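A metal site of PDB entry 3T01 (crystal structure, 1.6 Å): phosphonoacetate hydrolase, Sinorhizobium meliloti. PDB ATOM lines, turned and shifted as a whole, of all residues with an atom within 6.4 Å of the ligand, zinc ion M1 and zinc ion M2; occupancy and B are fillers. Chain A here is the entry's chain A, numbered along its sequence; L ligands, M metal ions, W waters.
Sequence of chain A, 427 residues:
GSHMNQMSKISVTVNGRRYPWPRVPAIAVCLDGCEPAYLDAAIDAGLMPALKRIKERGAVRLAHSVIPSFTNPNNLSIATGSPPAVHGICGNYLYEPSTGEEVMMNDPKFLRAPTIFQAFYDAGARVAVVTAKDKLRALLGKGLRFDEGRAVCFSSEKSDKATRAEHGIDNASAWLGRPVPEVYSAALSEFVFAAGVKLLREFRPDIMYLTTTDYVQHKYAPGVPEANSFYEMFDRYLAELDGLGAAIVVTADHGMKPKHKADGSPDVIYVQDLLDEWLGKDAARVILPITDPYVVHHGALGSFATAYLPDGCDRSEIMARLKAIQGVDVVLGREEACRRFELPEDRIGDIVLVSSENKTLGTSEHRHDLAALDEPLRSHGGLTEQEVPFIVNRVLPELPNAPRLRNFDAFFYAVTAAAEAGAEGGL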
ATOM      1  N   CYS A  30     -19.593 -22.765  -4.014  1.00  0.00           N
ATOM      2  CA  CYS A  30     -19.167 -21.544  -3.358  1.00  0.00           C
ATOM      3  C   CYS A  30     -18.128 -20.857  -4.229  1.00  0.00           C
ATOM      4  O   CYS A  30     -16.981 -21.310  -4.317  1.00  0.00           O
ATOM      5  CB  CYS A  30     -18.586 -21.851  -1.973  1.00  0.00           C
ATOM      6  SG  CYS A  30     -17.965 -20.391  -1.117  1.00  0.00           S
ATOM      7  N   ASP A  32     -15.838 -18.279  -4.190  1.00  0.00           N
ATOM      8  CA  ASP A  32     -15.121 -17.503  -3.183  1.00  0.00           C
ATOM      9  C   ASP A  32     -14.970 -16.049  -3.630  1.00  0.00           C
ATOM     10  O   ASP A  32     -14.473 -15.761  -4.716  1.00  0.00           O
ATOM     11  CB  ASP A  32     -13.763 -18.148  -2.924  1.00  0.00           C
ATOM     12  CG  ASP A  32     -13.177 -17.777  -1.582  1.00  0.00           C
ATOM     13  OD1 ASP A  32     -13.273 -16.600  -1.185  1.00  0.00           O
ATOM     14  OD2 ASP A  32     -12.612 -18.682  -0.932  1.00  0.00           O
ATOM     15  N   GLY A  33     -15.425 -15.125  -2.775  1.00  0.00           N
ATOM     16  CA  GLY A  33     -15.299 -13.701  -3.038  1.00  0.00           C
ATOM     17  C   GLY A  33     -16.129 -13.153  -4.189  1.00  0.00           C
ATOM     18  O   GLY A  33     -15.844 -12.057  -4.687  1.00  0.00           O
ATOM     19  N   SER A  69     -17.295 -11.537   7.294  1.00  0.00           N
ATOM     20  CA  SER A  69     -17.416 -12.032   5.914  1.00  0.00           C
ATOM     21  C   SER A  69     -16.068 -12.521   5.403  1.00  0.00           C
ATOM     22  O   SER A  69     -15.506 -11.985   4.437  1.00  0.00           O
ATOM     23  CB  SER A  69     -18.078 -10.981   5.013  1.00  0.00           C
ATOM     24  OG  SER A  69     -17.377  -9.742   5.033  1.00  0.00           O
ATOM     25  N   PHE A  70     -15.561 -13.557   6.069  1.00  0.00           N
ATOM     26  CA  PHE A  70     -14.293 -14.204   5.735  1.00  0.00           C
ATOM     27  C   PHE A  70     -14.535 -15.647   5.262  1.00  0.00           C
ATOM     28  O   PHE A  70     -15.622 -16.196   5.452  1.00  0.00           O
ATOM     29  CB  PHE A  70     -13.335 -14.218   6.928  1.00  0.00           C
ATOM     30  CG  PHE A  70     -12.813 -12.846   7.330  1.00  0.00           C
ATOM     31  CD1 PHE A  70     -12.397 -11.920   6.377  1.00  0.00           C
ATOM     32  CD2 PHE A  70     -12.710 -12.518   8.675  1.00  0.00           C
ATOM     33  CE1 PHE A  70     -11.915 -10.662   6.767  1.00  0.00           C
ATOM     34  CE2 PHE A  70     -12.225 -11.270   9.082  1.00  0.00           C
ATOM     35  CZ  PHE A  70     -11.833 -10.341   8.123  1.00  0.00           C
ATOM     36  N   THR A  71     -13.510 -16.234   4.663  1.00  0.00           N
ATOM     37  CA  THR A  71     -13.618 -17.529   3.998  1.00  0.00           C
ATOM     38  C   THR A  71     -13.936 -18.705   4.908  1.00  0.00           C
ATOM     39  O   THR A  71     -14.891 -19.449   4.641  1.00  0.00           O
ATOM     40  CB  THR A  71     -12.350 -17.824   3.180  1.00  0.00           C
ATOM     41  OG1 THR A  71     -12.224 -16.814   2.168  1.00  0.00           O
ATOM     42  CG2 THR A  71     -12.408 -19.213   2.522  1.00  0.00           C
ATOM     43  N   ASN A  72     -13.138 -18.890   5.958  1.00  0.00           N
ATOM     44  CA  ASN A  72     -13.327 -20.058   6.818  1.00  0.00           C
ATOM     45  C   ASN A  72     -14.671 -20.081   7.547  1.00  0.00           C
ATOM     46  O   ASN A  72     -15.379 -21.080   7.469  1.00  0.00           O
ATOM     47  CB  ASN A  72     -12.164 -20.256   7.792  1.00  0.00           C
ATOM     48  CG  ASN A  72     -10.873 -20.654   7.110  1.00  0.00           C
ATOM     49  OD1 ASN A  72     -10.575 -20.204   5.996  1.00  0.00           O
ATOM     50  ND2 ASN A  72     -10.079 -21.499   7.771  1.00  0.00           N
ATOM     51  N   PRO A  73     -15.040 -18.971   8.227  1.00  0.00           N
ATOM     52  CA  PRO A  73     -16.331 -19.000   8.933  1.00  0.00           C
ATOM     53  C   PRO A  73     -17.503 -19.233   7.981  1.00  0.00           C
ATOM     54  O   PRO A  73     -18.451 -19.955   8.319  1.00  0.00           O
ATOM     55  CB  PRO A  73     -16.431 -17.608   9.558  1.00  0.00           C
ATOM     56  CG  PRO A  73     -15.052 -17.090   9.595  1.00  0.00           C
ATOM     57  CD  PRO A  73     -14.333 -17.694   8.441  1.00  0.00           C
ATOM     58  N   ASN A  75     -17.429 -20.728   4.814  1.00  0.00           N
ATOM     59  CA  ASN A  75     -17.406 -22.090   4.275  1.00  0.00           C
ATOM     60  C   ASN A  75     -17.939 -23.109   5.274  1.00  0.00           C
ATOM     61  O   ASN A  75     -18.703 -24.003   4.904  1.00  0.00           O
ATOM     62  CB  ASN A  75     -16.021 -22.490   3.809  1.00  0.00           C
ATOM     63  CG  ASN A  75     -15.768 -22.077   2.379  1.00  0.00           C
ATOM     64  OD1 ASN A  75     -15.254 -20.979   2.102  1.00  0.00           O
ATOM     65  ND2 ASN A  75     -16.130 -22.938   1.455  1.00  0.00           N
ATOM     66  N   ASN A  92      -9.622 -17.543  11.520  1.00  0.00           N
ATOM     67  CA  ASN A  92      -8.539 -18.450  11.148  1.00  0.00           C
ATOM     68  C   ASN A  92      -7.729 -18.929  12.341  1.00  0.00           C
ATOM     69  O   ASN A  92      -7.076 -19.982  12.278  1.00  0.00           O
ATOM     70  CB  ASN A  92      -7.622 -17.803  10.098  1.00  0.00           C
ATOM     71  CG  ASN A  92      -8.251 -17.790   8.715  1.00  0.00           C
ATOM     72  OD1 ASN A  92      -9.349 -18.291   8.517  1.00  0.00           O
ATOM     73  ND2 ASN A  92      -7.534 -17.224   7.754  1.00  0.00           N
ATOM     74  N   LYS A 133      -8.059 -24.756  -1.993  1.00  0.00           N
ATOM     75  CA  LYS A 133      -6.968 -24.757  -1.035  1.00  0.00           C
ATOM     76  C   LYS A 133      -7.128 -25.892  -0.032  1.00  0.00           C
ATOM     77  O   LYS A 133      -8.247 -26.265   0.334  1.00  0.00           O
ATOM     78  CB  LYS A 133      -6.853 -23.399  -0.334  1.00  0.00           C
ATOM     79  CG  LYS A 133      -6.087 -22.360  -1.136  1.00  0.00           C
ATOM     80  CD  LYS A 133      -4.578 -22.516  -0.970  1.00  0.00           C
ATOM     81  CE  LYS A 133      -4.039 -21.641   0.167  1.00  0.00           C
ATOM     82  NZ  LYS A 133      -4.056 -20.191  -0.151  1.00  0.00           N
ATOM     83  N   LYS A 135      -6.111 -26.285   3.271  1.00  0.00           N
ATOM     84  CA  LYS A 135      -6.349 -26.117   4.705  1.00  0.00           C
ATOM     85  C   LYS A 135      -7.829 -26.169   5.079  1.00  0.00           C
ATOM     86  O   LYS A 135      -8.167 -26.352   6.246  1.00  0.00           O
ATOM     87  CB  LYS A 135      -5.654 -24.852   5.251  1.00  0.00           C
ATOM     88  CG  LYS A 135      -6.166 -23.512   4.737  1.00  0.00           C
ATOM     89  CD  LYS A 135      -7.123 -22.865   5.720  1.00  0.00           C
ATOM     90  CE  LYS A 135      -7.136 -21.360   5.548  1.00  0.00           C
ATOM     91  NZ  LYS A 135      -7.247 -20.973   4.113  1.00  0.00           N
ATOM     92  N   THR A 212     -13.999 -22.642  -4.028  1.00  0.00           N
ATOM     93  CA  THR A 212     -12.860 -22.126  -4.792  1.00  0.00           C
ATOM     94  C   THR A 212     -11.989 -21.242  -3.898  1.00  0.00           C
ATOM     95  O   THR A 212     -12.087 -21.331  -2.678  1.00  0.00           O
ATOM     96  CB  THR A 212     -13.386 -21.339  -6.004  1.00  0.00           C
ATOM     97  OG1 THR A 212     -14.216 -20.265  -5.553  1.00  0.00           O
ATOM     98  CG2 THR A 212     -14.220 -22.248  -6.907  1.00  0.00           C
ATOM     99  N   THR A 213     -11.107 -20.433  -4.490  1.00  0.00           N
ATOM    100  CA  THR A 213     -10.423 -19.378  -3.725  1.00  0.00           C
ATOM    101  C   THR A 213     -10.687 -18.034  -4.368  1.00  0.00           C
ATOM    102  O   THR A 213     -11.114 -17.969  -5.532  1.00  0.00           O
ATOM    103  CB  THR A 213      -8.877 -19.551  -3.597  1.00  0.00           C
ATOM    104  OG1 THR A 213      -8.236 -19.075  -4.784  1.00  0.00           O
ATOM    105  CG2 THR A 213      -8.501 -20.988  -3.338  1.00  0.00           C
ATOM    106  N   ASP A 214     -10.434 -16.967  -3.611  1.00  0.00           N
ATOM    107  CA  ASP A 214     -10.693 -15.615  -4.100  1.00  0.00           C
ATOM    108  C   ASP A 214      -9.436 -14.920  -4.628  1.00  0.00           C
ATOM    109  O   ASP A 214      -9.362 -13.691  -4.611  1.00  0.00           O
ATOM    110  CB  ASP A 214     -11.414 -14.770  -3.040  1.00  0.00           C
ATOM    111  CG  ASP A 214     -10.645 -14.639  -1.736  1.00  0.00           C
ATOM    112  OD1 ASP A 214      -9.522 -15.176  -1.600  1.00  0.00           O
ATOM    113  OD2 ASP A 214     -11.191 -13.991  -0.804  1.00  0.00           O
ATOM    114  N   HIS A 218      -9.436 -10.838  -5.339  1.00  0.00           N
ATOM    115  CA  HIS A 218      -8.588  -9.884  -4.611  1.00  0.00           C
ATOM    116  C   HIS A 218      -7.784  -9.014  -5.574  1.00  0.00           C
ATOM    117  O   HIS A 218      -7.468  -7.874  -5.250  1.00  0.00           O
ATOM    118  CB  HIS A 218      -7.639 -10.594  -3.653  1.00  0.00           C
ATOM    119  CG  HIS A 218      -8.224 -10.921  -2.308  1.00  0.00           C
ATOM    120  ND1 HIS A 218      -8.429  -9.989  -1.325  1.00  0.00           N
ATOM    121  CD2 HIS A 218      -8.625 -12.109  -1.786  1.00  0.00           C
ATOM    122  CE1 HIS A 218      -8.949 -10.565  -0.261  1.00  0.00           C
ATOM    123  NE2 HIS A 218      -9.066 -11.860  -0.507  1.00  0.00           N
ATOM    124  N   ASP A 253     -19.087 -17.276  -0.337  1.00  0.00           N
ATOM    125  CA  ASP A 253     -18.787 -17.140   1.077  1.00  0.00           C
ATOM    126  C   ASP A 253     -18.842 -15.685   1.569  1.00  0.00           C
ATOM    127  O   ASP A 253     -19.129 -15.430   2.724  1.00  0.00           O
ATOM    128  CB  ASP A 253     -17.459 -17.824   1.446  1.00  0.00           C
ATOM    129  CG  ASP A 253     -16.266 -17.296   0.657  1.00  0.00           C
ATOM    130  OD1 ASP A 253     -16.436 -16.585  -0.362  1.00  0.00           O
ATOM    131  OD2 ASP A 253     -15.138 -17.607   1.072  1.00  0.00           O
ATOM    132  N   HIS A 254     -18.564 -14.751   0.654  1.00  0.00           N
ATOM    133  CA  HIS A 254     -18.540 -13.315   0.926  1.00  0.00           C
ATOM    134  C   HIS A 254     -18.287 -12.596  -0.388  1.00  0.00           C
ATOM    135  O   HIS A 254     -17.898 -13.229  -1.391  1.00  0.00           O
ATOM    136  CB  HIS A 254     -17.410 -12.948   1.903  1.00  0.00           C
ATOM    137  CG  HIS A 254     -16.073 -13.437   1.463  1.00  0.00           C
ATOM    138  ND1 HIS A 254     -15.322 -12.806   0.499  1.00  0.00           N
ATOM    139  CD2 HIS A 254     -15.363 -14.532   1.843  1.00  0.00           C
ATOM    140  CE1 HIS A 254     -14.209 -13.482   0.301  1.00  0.00           C
ATOM    141  NE2 HIS A 254     -14.208 -14.535   1.093  1.00  0.00           N
ATOM    142  N   MET A 256     -16.667  -8.753  -2.229  1.00  0.00           N
ATOM    143  CA  MET A 256     -15.342  -8.165  -2.388  1.00  0.00           C
ATOM    144  C   MET A 256     -15.523  -6.695  -2.752  1.00  0.00           C
ATOM    145  O   MET A 256     -16.344  -6.356  -3.605  1.00  0.00           O
ATOM    146  CB  MET A 256     -14.550  -8.897  -3.486  1.00  0.00           C
ATOM    147  CG  MET A 256     -13.062  -8.519  -3.582  1.00  0.00           C
ATOM    148  SD  MET A 256     -12.041  -9.213  -2.253  1.00  0.00           S
ATOM    149  CE  MET A 256     -12.110 -10.967  -2.606  1.00  0.00           C
ATOM    150  N   PRO A 289      -8.811 -11.710  12.150  1.00  0.00           N
ATOM    151  CA  PRO A 289      -9.233 -13.071  11.809  1.00  0.00           C
ATOM    152  C   PRO A 289      -9.053 -13.505  10.347  1.00  0.00           C
ATOM    153  O   PRO A 289      -9.068 -14.707  10.081  1.00  0.00           O
ATOM    154  CB  PRO A 289     -10.734 -13.076  12.154  1.00  0.00           C
ATOM    155  CG  PRO A 289     -10.907 -11.940  13.109  1.00  0.00           C
ATOM    156  CD  PRO A 289      -9.940 -10.903  12.647  1.00  0.00           C
ATOM    157  N   ILE A 290      -8.863 -12.539   9.441  1.00  0.00           N
ATOM    158  CA  ILE A 290      -8.842 -12.811   7.992  1.00  0.00           C
ATOM    159  C   ILE A 290      -7.859 -13.899   7.567  1.00  0.00           C
ATOM    160  O   ILE A 290      -8.182 -14.722   6.705  1.00  0.00           O
ATOM    161  CB  ILE A 290      -8.606 -11.520   7.136  1.00  0.00           C
ATOM    162  CG1 ILE A 290      -8.748 -11.839   5.639  1.00  0.00           C
ATOM    163  CG2 ILE A 290      -7.263 -10.870   7.452  1.00  0.00           C
ATOM    164  CD1 ILE A 290      -8.868 -10.619   4.728  1.00  0.00           C
ATOM    165  N   THR A 291      -6.679 -13.915   8.166  1.00  0.00           N
ATOM    166  CA  THR A 291      -5.651 -14.895   7.807  1.00  0.00           C
ATOM    167  C   THR A 291      -4.885 -15.406   9.024  1.00  0.00           C
ATOM    168  O   THR A 291      -5.238 -15.089  10.166  1.00  0.00           O
ATOM    169  CB  THR A 291      -4.703 -14.350   6.694  1.00  0.00           C
ATOM    170  OG1 THR A 291      -3.873 -15.411   6.203  1.00  0.00           O
ATOM    171  CG2 THR A 291      -3.843 -13.213   7.223  1.00  0.00           C
ATOM    172  N   GLY A 299      -2.140  -9.256   2.644  1.00  0.00           N
ATOM    173  CA  GLY A 299      -3.164 -10.293   2.663  1.00  0.00           C
ATOM    174  C   GLY A 299      -3.787 -10.438   4.048  1.00  0.00           C
ATOM    175  O   GLY A 299      -4.746 -11.198   4.226  1.00  0.00           O
ATOM    176  N   SER A 379     -10.562  -6.223  -0.620  1.00  0.00           N
ATOM    177  CA  SER A 379     -10.753  -7.195   0.457  1.00  0.00           C
ATOM    178  C   SER A 379     -12.194  -7.323   0.920  1.00  0.00           C
ATOM    179  O   SER A 379     -13.134  -6.867   0.268  1.00  0.00           O
ATOM    180  CB  SER A 379      -9.807  -6.927   1.627  1.00  0.00           C
ATOM    181  OG  SER A 379      -9.567  -8.111   2.377  1.00  0.00           O
ATOM    182  N   HIS A 380     -12.352  -7.959   2.080  1.00  0.00           N
ATOM    183  CA  HIS A 380     -13.663  -8.300   2.599  1.00  0.00           C
ATOM    184  C   HIS A 380     -13.583  -8.422   4.121  1.00  0.00           C
ATOM    185  O   HIS A 380     -12.565  -8.037   4.719  1.00  0.00           O
ATOM    186  CB  HIS A 380     -14.152  -9.598   1.956  1.00  0.00           C
ATOM    187  CG  HIS A 380     -13.148 -10.700   1.961  1.00  0.00           C
ATOM    188  ND1 HIS A 380     -13.146 -11.696   2.913  1.00  0.00           N
ATOM    189  CD2 HIS A 380     -12.087 -10.957   1.150  1.00  0.00           C
ATOM    190  CE1 HIS A 380     -12.139 -12.525   2.679  1.00  0.00           C
ATOM    191  NE2 HIS A 380     -11.482 -12.094   1.615  1.00  0.00           N
HETATM  192  C1  LIG L   1      -9.829 -15.494   3.995  1.00  0.00           C
HETATM  193  O1  LIG L   1      -7.689 -15.894   2.611  1.00  0.00           O
HETATM  194  O2  LIG L   1      -9.216 -13.982   1.953  1.00  0.00           O
HETATM  195  O3  LIG L   1      -9.931 -16.380   1.586  1.00  0.00           O
HETATM  196  O4  LIG L   1      -9.276 -16.209   4.861  1.00  0.00           O
HETATM  197  O5  LIG L   1     -10.876 -14.873   4.256  1.00  0.00           O
HETATM  198  P1  LIG L   1      -9.113 -15.424   2.425  1.00  0.00           P
HETATM  199 ZN    ZN M   1     -10.096 -13.224   0.604  1.00  0.00          ZN
HETATM  200 ZN    ZN M   2     -13.521 -16.400   0.723  1.00  0.00          ZN
HETATM  201  O   HOH W   1      -9.035 -18.842   4.282  1.00  0.00           O
HETATM  202  O   HOH W   2      -6.589 -16.525   4.962  1.00  0.00           O
HETATM  203  O   HOH W   3     -10.040 -17.978  -0.647  1.00  0.00           O
HETATM  204  O   HOH W   4     -11.049 -17.213   6.815  1.00  0.00           O
HETATM  205  O   HOH W   5      -6.589 -12.070   1.943  1.00  0.00           O
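The backbone NH (N) of Thr 71 sits at hydrogen-bond distance from an oxygen (O5) of the ligand.
An oxygen (O3) of the ligand lies close to the side-chain hydroxyl (OG1) of Thr 71 (2.4 Å).
An oxygen (O4) of the ligand sits close to the backbone carbonyl oxygen (O) of Ile 290 (2.6 Å).
OG1 of Thr 212 is in hydrogen-bond range of N of Asp 32 (2.9 Å).
The side-chain amide oxygen (OD1) of Asn 75 lies close to the backbone carbonyl oxygen (O) of Thr 71, 3.0 Å away.
A ring nitrogen (ND1) of His 254 lies close to a ring nitrogen (ND1) of His 380 (3.4 Å).
O of His 254 lies close to N of Gly 33, 3.4 Å away.
OD1 of Asp 253 sits at hydrogen-bond distance from N of Gly 33 (3.0 Å).
The backbone carbonyl oxygen (O) of Ser 69 sits at hydrogen-bond distance from a ring nitrogen (ND1) of His 380.
The side-chain amide nitrogen (ND2) of Asn 92 is in hydrogen-bond range of the backbone carbonyl oxygen (O) of Ile 290 (2.8 Å).
The side-chain amide oxygen of Asn 92 lies close to the side-chain amide nitrogen of Asn 72, at 3.4 Å.
Phe 70 touches the ligand.
Asn 92 touches the ligand.
Hydrophobic or aromatic side chains within 4 Å of the ligand: Phe 70, Ile 290 and His 380.
Seven residues have an atom within 4 Å of the ligand: Phe 70, Thr 71, Asn 92, Asp 214, His 218, Ile 290 and His 380.
The nearest printed residue that does not touch the ligand is Asp 32 (4.3 Å).
Within 4 Å of zinc ion M1: Asp 214, His 218 and His 380.
Along chain A the residues within 4 Å of zinc ion M1 span positions 214 to 380.
The nearest printed residue that does not touch zinc ion M1 is His 254 (4.1 Å).
Of the 25 residues printed, 5 come within 4 Å of zinc ion M2.
The nearest printed residue that does not touch zinc ion M2 is Gly 33 (4.2 Å).
An oxygen (O2) of the ligand is bound to zinc ion M1 (1.8 Å).
OD2 of Asp 214 binds zinc ion M1, 1.9 Å away.
NE2 of His 218 is bound to zinc ion M1 (2.0 Å).
NE2 of His 380 binds zinc ion M1.
Zinc ion M2 is bound by the side-chain carboxylate (OD1) of Asp 32 (1.9 Å).
Zinc ion M2 is bound by OG1 of Thr 71 (2.0 Å).
Zinc ion M2 is bound by NE2 of His 254, 2.0 Å away.
OD2 of Asp 253 is bound to zinc ion M2, 2.0 Å away.
Water W2 lies within hydrogen-bond range of O1 of the ligand, O of Ile 290, ND2 of Asn 92 and OG1 of Thr 291.
Water W1 lies within hydrogen-bond range of the side-chain amide oxygen (OD1) of Asn 72, an oxygen (O4) of the ligand and the side-chain amino group (NZ) of Lys 135.
Water W3 lies within hydrogen-bond range of the side-chain carboxylate of Asp 32 (2.7 Å), an oxygen (O3) of the ligand (2.7 Å) and the side-chain carboxylate of Asp 214 (3.0 Å).
Water W4 lies within hydrogen-bond range of OD1 of Asn 92 (2.6 Å), N of Asn 72 (2.8 Å), O4 of the ligand (2.8 Å) and N of Thr 71 (3.4 Å).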
